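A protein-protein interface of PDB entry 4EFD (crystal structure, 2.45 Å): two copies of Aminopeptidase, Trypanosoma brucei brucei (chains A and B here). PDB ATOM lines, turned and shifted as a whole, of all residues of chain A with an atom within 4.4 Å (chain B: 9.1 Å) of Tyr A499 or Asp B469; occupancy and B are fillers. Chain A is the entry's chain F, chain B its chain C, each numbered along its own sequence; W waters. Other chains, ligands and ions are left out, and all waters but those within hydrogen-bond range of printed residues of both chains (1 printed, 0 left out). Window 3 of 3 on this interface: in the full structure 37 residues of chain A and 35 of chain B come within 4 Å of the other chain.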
ATOM      1  N   LEU A 301     -22.627 -25.002  17.374  1.00  0.00           N
ATOM      2  CA  LEU A 301     -22.346 -23.702  17.986  1.00  0.00           C
ATOM      3  C   LEU A 301     -21.421 -23.848  19.193  1.00  0.00           C
ATOM      4  O   LEU A 301     -21.103 -24.962  19.615  1.00  0.00           O
ATOM      5  CB  LEU A 301     -23.651 -23.023  18.414  1.00  0.00           C
ATOM      6  CG  LEU A 301     -24.719 -22.842  17.332  1.00  0.00           C
ATOM      7  CD1 LEU A 301     -26.030 -22.391  17.957  1.00  0.00           C
ATOM      8  CD2 LEU A 301     -24.257 -21.853  16.271  1.00  0.00           C
ATOM      9  N   LEU A 309     -29.748 -20.231  23.974  1.00  0.00           N
ATOM     10  CA  LEU A 309     -30.872 -20.983  23.395  1.00  0.00           C
ATOM     11  C   LEU A 309     -31.654 -21.789  24.441  1.00  0.00           C
ATOM     12  O   LEU A 309     -32.825 -22.104  24.230  1.00  0.00           O
ATOM     13  CB  LEU A 309     -30.387 -21.919  22.278  1.00  0.00           C
ATOM     14  CG  LEU A 309     -30.210 -21.301  20.889  1.00  0.00           C
ATOM     15  CD1 LEU A 309     -29.217 -20.148  20.910  1.00  0.00           C
ATOM     16  CD2 LEU A 309     -29.773 -22.364  19.892  1.00  0.00           C
ATOM     17  N   GLY A 405     -28.844 -26.113  17.030  1.00  0.00           N
ATOM     18  CA  GLY A 405     -28.292 -24.819  16.640  1.00  0.00           C
ATOM     19  C   GLY A 405     -28.081 -24.735  15.139  1.00  0.00           C
ATOM     20  O   GLY A 405     -28.035 -23.640  14.574  1.00  0.00           O
ATOM     21  N   GLN A 407     -30.217 -25.479  12.975  1.00  0.00           N
ATOM     22  CA  GLN A 407     -31.443 -24.902  12.423  1.00  0.00           C
ATOM     23  C   GLN A 407     -31.268 -23.420  12.082  1.00  0.00           C
ATOM     24  O   GLN A 407     -31.749 -22.958  11.045  1.00  0.00           O
ATOM     25  CB  GLN A 407     -32.605 -25.089  13.401  1.00  0.00           C
ATOM     26  CG  GLN A 407     -33.950 -24.608  12.876  1.00  0.00           C
ATOM     27  CD  GLN A 407     -34.207 -23.136  13.159  1.00  0.00           C
ATOM     28  OE1 GLN A 407     -34.312 -22.729  14.312  1.00  0.00           O
ATOM     29  NE2 GLN A 407     -34.313 -22.337  12.103  1.00  0.00           N
ATOM     30  N   GLY A 408     -30.588 -22.686  12.958  1.00  0.00           N
ATOM     31  CA  GLY A 408     -30.316 -21.269  12.733  1.00  0.00           C
ATOM     32  C   GLY A 408     -29.404 -21.052  11.540  1.00  0.00           C
ATOM     33  O   GLY A 408     -29.674 -20.207  10.687  1.00  0.00           O
ATOM     34  N   ILE A 409     -28.329 -21.831  11.477  1.00  0.00           N
ATOM     35  CA  ILE A 409     -27.385 -21.759  10.364  1.00  0.00           C
ATOM     36  C   ILE A 409     -28.035 -22.180   9.040  1.00  0.00           C
ATOM     37  O   ILE A 409     -27.691 -21.649   7.983  1.00  0.00           O
ATOM     38  CB  ILE A 409     -26.138 -22.638  10.624  1.00  0.00           C
ATOM     39  CG1 ILE A 409     -25.359 -22.123  11.839  1.00  0.00           C
ATOM     40  CG2 ILE A 409     -25.223 -22.653   9.402  1.00  0.00           C
ATOM     41  CD1 ILE A 409     -24.333 -23.105  12.362  1.00  0.00           C
ATOM     42  N   GLY A 412     -32.494 -20.204   9.403  1.00  0.00           N
ATOM     43  CA  GLY A 412     -32.507 -18.837   9.933  1.00  0.00           C
ATOM     44  C   GLY A 412     -33.450 -18.575  11.093  1.00  0.00           C
ATOM     45  O   GLY A 412     -34.068 -19.494  11.631  1.00  0.00           O
ATOM     46  N   ARG A 413     -33.559 -17.298  11.464  1.00  0.00           N
ATOM     47  CA  ARG A 413     -34.279 -16.870  12.670  1.00  0.00           C
ATOM     48  C   ARG A 413     -35.800 -16.850  12.517  1.00  0.00           C
ATOM     49  O   ARG A 413     -36.519 -16.848  13.517  1.00  0.00           O
ATOM     50  CB  ARG A 413     -33.822 -15.465  13.099  1.00  0.00           C
ATOM     51  CG  ARG A 413     -32.343 -15.334  13.452  1.00  0.00           C
ATOM     52  CD  ARG A 413     -32.000 -16.108  14.708  1.00  0.00           C
ATOM     53  NE  ARG A 413     -30.623 -15.887  15.162  1.00  0.00           N
ATOM     54  CZ  ARG A 413     -30.242 -15.007  16.092  1.00  0.00           C
ATOM     55  NH1 ARG A 413     -28.955 -14.914  16.415  1.00  0.00           N
ATOM     56  NH2 ARG A 413     -31.124 -14.219  16.704  1.00  0.00           N
ATOM     57  N   LEU A 497     -37.765 -25.719  15.586  1.00  0.00           N
ATOM     58  CA  LEU A 497     -38.081 -24.307  15.792  1.00  0.00           C
ATOM     59  C   LEU A 497     -37.209 -23.698  16.897  1.00  0.00           C
ATOM     60  O   LEU A 497     -37.690 -22.940  17.737  1.00  0.00           O
ATOM     61  CB  LEU A 497     -39.579 -24.131  16.092  1.00  0.00           C
ATOM     62  CG  LEU A 497     -40.289 -25.149  16.995  1.00  0.00           C
ATOM     63  CD1 LEU A 497     -39.709 -25.177  18.402  1.00  0.00           C
ATOM     64  CD2 LEU A 497     -41.779 -24.847  17.037  1.00  0.00           C
ATOM     65  N   ALA A 498     -35.918 -24.017  16.867  1.00  0.00           N
ATOM     66  CA  ALA A 498     -34.971 -23.541  17.876  1.00  0.00           C
ATOM     67  C   ALA A 498     -34.905 -22.016  17.950  1.00  0.00           C
ATOM     68  O   ALA A 498     -34.852 -21.446  19.041  1.00  0.00           O
ATOM     69  CB  ALA A 498     -33.584 -24.114  17.608  1.00  0.00           C
ATOM     70  N   TYR A 499     -34.907 -21.367  16.788  1.00  0.00           N
ATOM     71  CA  TYR A 499     -34.758 -19.910  16.705  1.00  0.00           C
ATOM     72  C   TYR A 499     -36.059 -19.102  16.535  1.00  0.00           C
ATOM     73  O   TYR A 499     -36.215 -18.068  17.183  1.00  0.00           O
ATOM     74  CB  TYR A 499     -33.748 -19.552  15.611  1.00  0.00           C
ATOM     75  CG  TYR A 499     -32.314 -19.777  16.037  1.00  0.00           C
ATOM     76  CD1 TYR A 499     -31.570 -18.749  16.609  1.00  0.00           C
ATOM     77  CD2 TYR A 499     -31.704 -21.020  15.884  1.00  0.00           C
ATOM     78  CE1 TYR A 499     -30.255 -18.947  17.006  1.00  0.00           C
ATOM     79  CE2 TYR A 499     -30.390 -21.229  16.281  1.00  0.00           C
ATOM     80  CZ  TYR A 499     -29.671 -20.188  16.840  1.00  0.00           C
ATOM     81  OH  TYR A 499     -28.368 -20.382  17.234  1.00  0.00           O
ATOM     82  N   PRO A 500     -36.992 -19.556  15.673  1.00  0.00           N
ATOM     83  CA  PRO A 500     -38.248 -18.806  15.488  1.00  0.00           C
ATOM     84  C   PRO A 500     -39.115 -18.636  16.746  1.00  0.00           C
ATOM     85  O   PRO A 500     -40.001 -17.781  16.764  1.00  0.00           O
ATOM     86  CB  PRO A 500     -38.996 -19.635  14.439  1.00  0.00           C
ATOM     87  CG  PRO A 500     -37.939 -20.357  13.704  1.00  0.00           C
ATOM     88  CD  PRO A 500     -36.893 -20.674  14.718  1.00  0.00           C
ATOM     89  N   VAL A 501     -38.853 -19.436  17.779  1.00  0.00           N
ATOM     90  CA  VAL A 501     -39.585 -19.362  19.048  1.00  0.00           C
ATOM     91  C   VAL A 501     -39.288 -18.112  19.874  1.00  0.00           C
ATOM     92  O   VAL A 501     -39.999 -17.832  20.837  1.00  0.00           O
ATOM     93  CB  VAL A 501     -39.328 -20.642  19.928  1.00  0.00           C
ATOM     94  CG1 VAL A 501     -37.893 -21.124  19.910  1.00  0.00           C
ATOM     95  CG2 VAL A 501     -40.037 -20.647  21.217  1.00  0.00           C
ATOM     96  N   PHE A 502     -38.256 -17.358  19.502  1.00  0.00           N
ATOM     97  CA  PHE A 502     -37.887 -16.164  20.257  1.00  0.00           C
ATOM     98  C   PHE A 502     -37.312 -15.045  19.389  1.00  0.00           C
ATOM     99  O   PHE A 502     -36.945 -15.256  18.233  1.00  0.00           O
ATOM    100  CB  PHE A 502     -36.878 -16.533  21.351  1.00  0.00           C
ATOM    101  CG  PHE A 502     -35.474 -16.736  20.846  1.00  0.00           C
ATOM    102  CD1 PHE A 502     -34.568 -15.681  20.836  1.00  0.00           C
ATOM    103  CD2 PHE A 502     -35.056 -17.979  20.385  1.00  0.00           C
ATOM    104  CE1 PHE A 502     -33.271 -15.859  20.371  1.00  0.00           C
ATOM    105  CE2 PHE A 502     -33.761 -18.166  19.922  1.00  0.00           C
ATOM    106  CZ  PHE A 502     -32.867 -17.104  19.913  1.00  0.00           C
ATOM    107  N   LEU B 299     -17.270 -18.151   9.923  1.00  0.00           N
ATOM    108  CA  LEU B 299     -17.515 -18.127  11.368  1.00  0.00           C
ATOM    109  C   LEU B 299     -18.236 -19.375  11.894  1.00  0.00           C
ATOM    110  O   LEU B 299     -18.169 -19.667  13.090  1.00  0.00           O
ATOM    111  CB  LEU B 299     -18.322 -16.878  11.736  1.00  0.00           C
ATOM    112  N   ALA B 300     -18.918 -20.104  11.011  1.00  0.00           N
ATOM    113  CA  ALA B 300     -19.725 -21.264  11.410  1.00  0.00           C
ATOM    114  C   ALA B 300     -18.886 -22.411  11.974  1.00  0.00           C
ATOM    115  O   ALA B 300     -19.298 -23.069  12.933  1.00  0.00           O
ATOM    116  CB  ALA B 300     -20.562 -21.756  10.232  1.00  0.00           C
ATOM    117  N   ALA B 406     -21.147 -23.420   6.363  1.00  0.00           N
ATOM    118  CA  ALA B 406     -22.565 -23.574   6.703  1.00  0.00           C
ATOM    119  C   ALA B 406     -23.315 -24.501   5.742  1.00  0.00           C
ATOM    120  O   ALA B 406     -24.342 -25.075   6.105  1.00  0.00           O
ATOM    121  CB  ALA B 406     -23.244 -22.212   6.734  1.00  0.00           C
ATOM    122  N   ILE B 409     -23.425 -28.012   7.124  1.00  0.00           N
ATOM    123  CA  ILE B 409     -24.385 -28.084   8.225  1.00  0.00           C
ATOM    124  C   ILE B 409     -25.821 -28.084   7.697  1.00  0.00           C
ATOM    125  O   ILE B 409     -26.694 -28.753   8.254  1.00  0.00           O
ATOM    126  CB  ILE B 409     -24.185 -26.916   9.225  1.00  0.00           C
ATOM    127  CG1 ILE B 409     -22.834 -27.050   9.935  1.00  0.00           C
ATOM    128  CG2 ILE B 409     -25.305 -26.881  10.256  1.00  0.00           C
ATOM    129  CD1 ILE B 409     -22.386 -25.791  10.651  1.00  0.00           C
ATOM    130  N   GLU B 453     -28.541  -8.370   7.667  1.00  0.00           N
ATOM    131  CA  GLU B 453     -27.302  -8.967   8.180  1.00  0.00           C
ATOM    132  C   GLU B 453     -26.028  -8.323   7.623  1.00  0.00           C
ATOM    133  O   GLU B 453     -24.967  -8.435   8.237  1.00  0.00           O
ATOM    134  CB  GLU B 453     -27.269 -10.472   7.891  1.00  0.00           C
ATOM    135  CG  GLU B 453     -28.319 -11.290   8.642  1.00  0.00           C
ATOM    136  CD  GLU B 453     -28.145 -11.246  10.153  1.00  0.00           C
ATOM    137  OE1 GLU B 453     -29.154 -11.416  10.866  1.00  0.00           O
ATOM    138  OE2 GLU B 453     -27.007 -11.043  10.633  1.00  0.00           O
ATOM    139  N   MET B 465     -22.177 -11.594   7.090  1.00  0.00           N
ATOM    140  CA  MET B 465     -23.362 -11.469   7.934  1.00  0.00           C
ATOM    141  C   MET B 465     -22.978 -11.249   9.398  1.00  0.00           C
ATOM    142  O   MET B 465     -22.023 -11.844   9.889  1.00  0.00           O
ATOM    143  CB  MET B 465     -24.243 -12.716   7.795  1.00  0.00           C
ATOM    144  CG  MET B 465     -23.584 -14.009   8.247  1.00  0.00           C
ATOM    145  SD  MET B 465     -24.417 -15.472   7.616  1.00  0.00           S
ATOM    146  CE  MET B 465     -26.066 -15.254   8.282  1.00  0.00           C
ATOM    147  N   GLU B 466     -23.731 -10.392  10.082  1.00  0.00           N
ATOM    148  CA  GLU B 466     -23.442 -10.044  11.475  1.00  0.00           C
ATOM    149  C   GLU B 466     -23.643 -11.271  12.363  1.00  0.00           C
ATOM    150  O   GLU B 466     -22.729 -11.689  13.073  1.00  0.00           O
ATOM    151  CB  GLU B 466     -24.336  -8.887  11.949  1.00  0.00           C
ATOM    152  CG  GLU B 466     -23.628  -7.827  12.797  1.00  0.00           C
ATOM    153  CD  GLU B 466     -23.127  -8.349  14.133  1.00  0.00           C
ATOM    154  OE1 GLU B 466     -23.726  -7.999  15.172  1.00  0.00           O
ATOM    155  OE2 GLU B 466     -22.127  -9.100  14.152  1.00  0.00           O
ATOM    156  N   ARG B 467     -24.838 -11.852  12.296  1.00  0.00           N
ATOM    157  CA  ARG B 467     -25.177 -13.040  13.076  1.00  0.00           C
ATOM    158  C   ARG B 467     -24.930 -14.299  12.247  1.00  0.00           C
ATOM    159  O   ARG B 467     -25.399 -14.402  11.116  1.00  0.00           O
ATOM    160  CB  ARG B 467     -26.637 -12.970  13.531  1.00  0.00           C
ATOM    161  CG  ARG B 467     -26.950 -11.740  14.374  1.00  0.00           C
ATOM    162  CD  ARG B 467     -28.402 -11.699  14.828  1.00  0.00           C
ATOM    163  NE  ARG B 467     -29.326 -11.456  13.720  1.00  0.00           N
ATOM    164  CZ  ARG B 467     -30.637 -11.261  13.854  1.00  0.00           C
ATOM    165  NH1 ARG B 467     -31.210 -11.273  15.055  1.00  0.00           N
ATOM    166  NH2 ARG B 467     -31.387 -11.049  12.777  1.00  0.00           N
ATOM    167  N   ARG B 468     -24.193 -15.250  12.814  1.00  0.00           N
ATOM    168  CA  ARG B 468     -23.807 -16.472  12.100  1.00  0.00           C
ATOM    169  C   ARG B 468     -24.976 -17.436  11.883  1.00  0.00           C
ATOM    170  O   ARG B 468     -25.003 -18.174  10.894  1.00  0.00           O
ATOM    171  CB  ARG B 468     -22.691 -17.195  12.858  1.00  0.00           C
ATOM    172  N   ASP B 469     -25.940 -17.415  12.800  1.00  0.00           N
ATOM    173  CA  ASP B 469     -27.041 -18.379  12.804  1.00  0.00           C
ATOM    174  C   ASP B 469     -28.332 -17.783  12.233  1.00  0.00           C
ATOM    175  O   ASP B 469     -29.386 -17.814  12.875  1.00  0.00           O
ATOM    176  CB  ASP B 469     -27.255 -18.944  14.222  1.00  0.00           C
ATOM    177  CG  ASP B 469     -27.184 -17.874  15.307  1.00  0.00           C
ATOM    178  OD1 ASP B 469     -26.927 -18.232  16.477  1.00  0.00           O
ATOM    179  OD2 ASP B 469     -27.374 -16.678  14.991  1.00  0.00           O
ATOM    180  N   ASN B 470     -28.240 -17.251  11.014  1.00  0.00           N
ATOM    181  CA  ASN B 470     -29.400 -16.699  10.313  1.00  0.00           C
ATOM    182  C   ASN B 470     -29.348 -16.998   8.808  1.00  0.00           C
ATOM    183  O   ASN B 470     -29.332 -16.087   7.974  1.00  0.00           O
ATOM    184  CB  ASN B 470     -29.514 -15.191  10.576  1.00  0.00           C
ATOM    185  CG  ASN B 470     -30.885 -14.630  10.219  1.00  0.00           C
ATOM    186  OD1 ASN B 470     -31.870 -15.366  10.127  1.00  0.00           O
ATOM    187  ND2 ASN B 470     -30.953 -13.317  10.024  1.00  0.00           N
ATOM    188  N   ALA B 471     -29.324 -18.288   8.478  1.00  0.00           N
ATOM    189  CA  ALA B 471     -29.269 -18.761   7.089  1.00  0.00           C
ATOM    190  C   ALA B 471     -27.957 -18.354   6.421  1.00  0.00           C
ATOM    191  O   ALA B 471     -27.933 -17.477   5.558  1.00  0.00           O
ATOM    192  CB  ALA B 471     -30.469 -18.253   6.293  1.00  0.00           C
ATOM    193  N   GLY B 472     -26.875 -19.008   6.832  1.00  0.00           N
ATOM    194  CA  GLY B 472     -25.527 -18.668   6.380  1.00  0.00           C
ATOM    195  C   GLY B 472     -25.286 -18.886   4.901  1.00  0.00           C
ATOM    196  O   GLY B 472     -24.663 -18.053   4.240  1.00  0.00           O
ATOM    197  N   VAL B 473     -25.777 -20.006   4.380  1.00  0.00           N
ATOM    198  CA  VAL B 473     -25.649 -20.304   2.957  1.00  0.00           C
ATOM    199  C   VAL B 473     -26.427 -19.276   2.140  1.00  0.00           C
ATOM    200  O   VAL B 473     -25.929 -18.766   1.134  1.00  0.00           O
ATOM    201  CB  VAL B 473     -26.174 -21.715   2.610  1.00  0.00           C
ATOM    202  CG1 VAL B 473     -25.884 -22.044   1.154  1.00  0.00           C
ATOM    203  CG2 VAL B 473     -25.551 -22.762   3.523  1.00  0.00           C
ATOM    204  N   CYS B 475     -27.374 -16.146   3.009  1.00  0.00           N
ATOM    205  CA  CYS B 475     -26.842 -14.788   3.109  1.00  0.00           C
ATOM    206  C   CYS B 475     -25.622 -14.597   2.210  1.00  0.00           C
ATOM    207  O   CYS B 475     -25.536 -13.609   1.482  1.00  0.00           O
ATOM    208  CB  CYS B 475     -26.505 -14.438   4.562  1.00  0.00           C
ATOM    209  SG  CYS B 475     -27.964 -14.174   5.600  1.00  0.00           S
HETATM  210  O   HOH W   1     -27.253 -18.013  19.163  1.00  0.00           O
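OD1 of Asn B470 is in hydrogen-bond range of N of Arg A413. The guanidinium group of Arg A413 lies close to the guanidinium group of Arg B467 (3.4 Å). The side-chain carboxylate (OD2) of Asp B469 is in salt-bridge range of the guanidinium group (NH1) of Arg A413, 2.8 Å away. N of Ala B471 sits at hydrogen-bond distance from O of Gly A408, 2.9 Å away. O of Asp B469 sits close to O of Gly A408. O of Ile A409 sits at hydrogen-bond distance from N of Gly B472 (3.0 Å). The side-chain carboxylate of Asp B469 is in hydrogen-bond range of the side-chain hydroxyl of Tyr A499, at 2.7 Å. The backbone NH (N) of Asn B470 is in hydrogen-bond range of the backbone carbonyl oxygen (O) of Gly A408, at 3.3 Å.
O of Ala B471 sits at hydrogen-bond distance from SG of Cys B475, 3.3 Å away. The side-chain sulfur of Cys B475 lies within hydrogen-bond range of the backbone carbonyl oxygen of Asn B470, 3.3 Å away. NE2 of Gln A407 is in hydrogen-bond range of O of Gly A412 (2.9 Å). OE1 of Glu B453 is in salt-bridge range of NE of Arg B467, at 2.9 Å. The side-chain amide oxygen (OE1) of Gln A407 is in hydrogen-bond range of the backbone NH (N) of Tyr A499. The side-chain carboxylate (OE1) of Glu B453 sits at hydrogen-bond distance from the side-chain amide nitrogen (ND2) of Asn B470, at 2.7 Å.
Among the printed residues, merely in contact across the chains: Ile A409 with Ala B406, Ile A409 with Ala B471, Gly A412 with Asn B470, Gly A412 with Ala B471, Ile A409 with Ile B409 and Ile A409 with Asp B469.
Printed residues of chain B within 4 Å of Tyr A499: Asp B469 (2.7 Å). Printed residues of chain A within 4 Å of Asp B469: Gly A408 (3.2 Å), Ile A409 (3.9 Å), Arg A413 (2.8 Å) and Tyr A499 (2.7 Å). Gly A408 touches just these residues of chain B: Asp B469 (3.2 Å), Asn B470 (3.3 Å) and Ala B471 (2.9 Å). No residue of chain B comes within 4 Å of Ala A498. No residue of chain B comes within 4 Å of Phe A502. Of the printed residues of chain A, Ala B471 touches Gly A408 (2.9 Å), Ile A409 (3.4 Å) and Gly A412 (3.5 Å). Printed residues of chain A within 4 Å of Ile B409: Ile A409. Ala B300 touches none of the printed residues of chain A. The nearest printed residue of chain A that does not touch Asp B469 is Gly A412 (4.4 Å). The nearest printed residue of chain A that does not touch Ala B471 is Arg A413 (5.3 Å).
Printed residues of chain A that touch a printed residue of chain B: Gly A408, Ile A409, Gly A412, Arg A413 and Tyr A499. Of the 15 printed residues of chain B, 7 touch a printed residue of chain A. Along chain B the printed residues that touch a printed residue of chain A span positions 406 to 472. Among the printed residues, 14 pairs touch across the chains.
Ile A409 touches its own counterpart, Ile B409. Position printed for both chains: 409. Of the 14 pairs that touch across the chains among the printed residues, 1 has its exchanged pair printed and touching as well.
Water W1 bridges the side-chain carboxylate of Asp B469 (2.7 Å) and the side-chain hydroxyl of Tyr A499 (3.3 Å).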
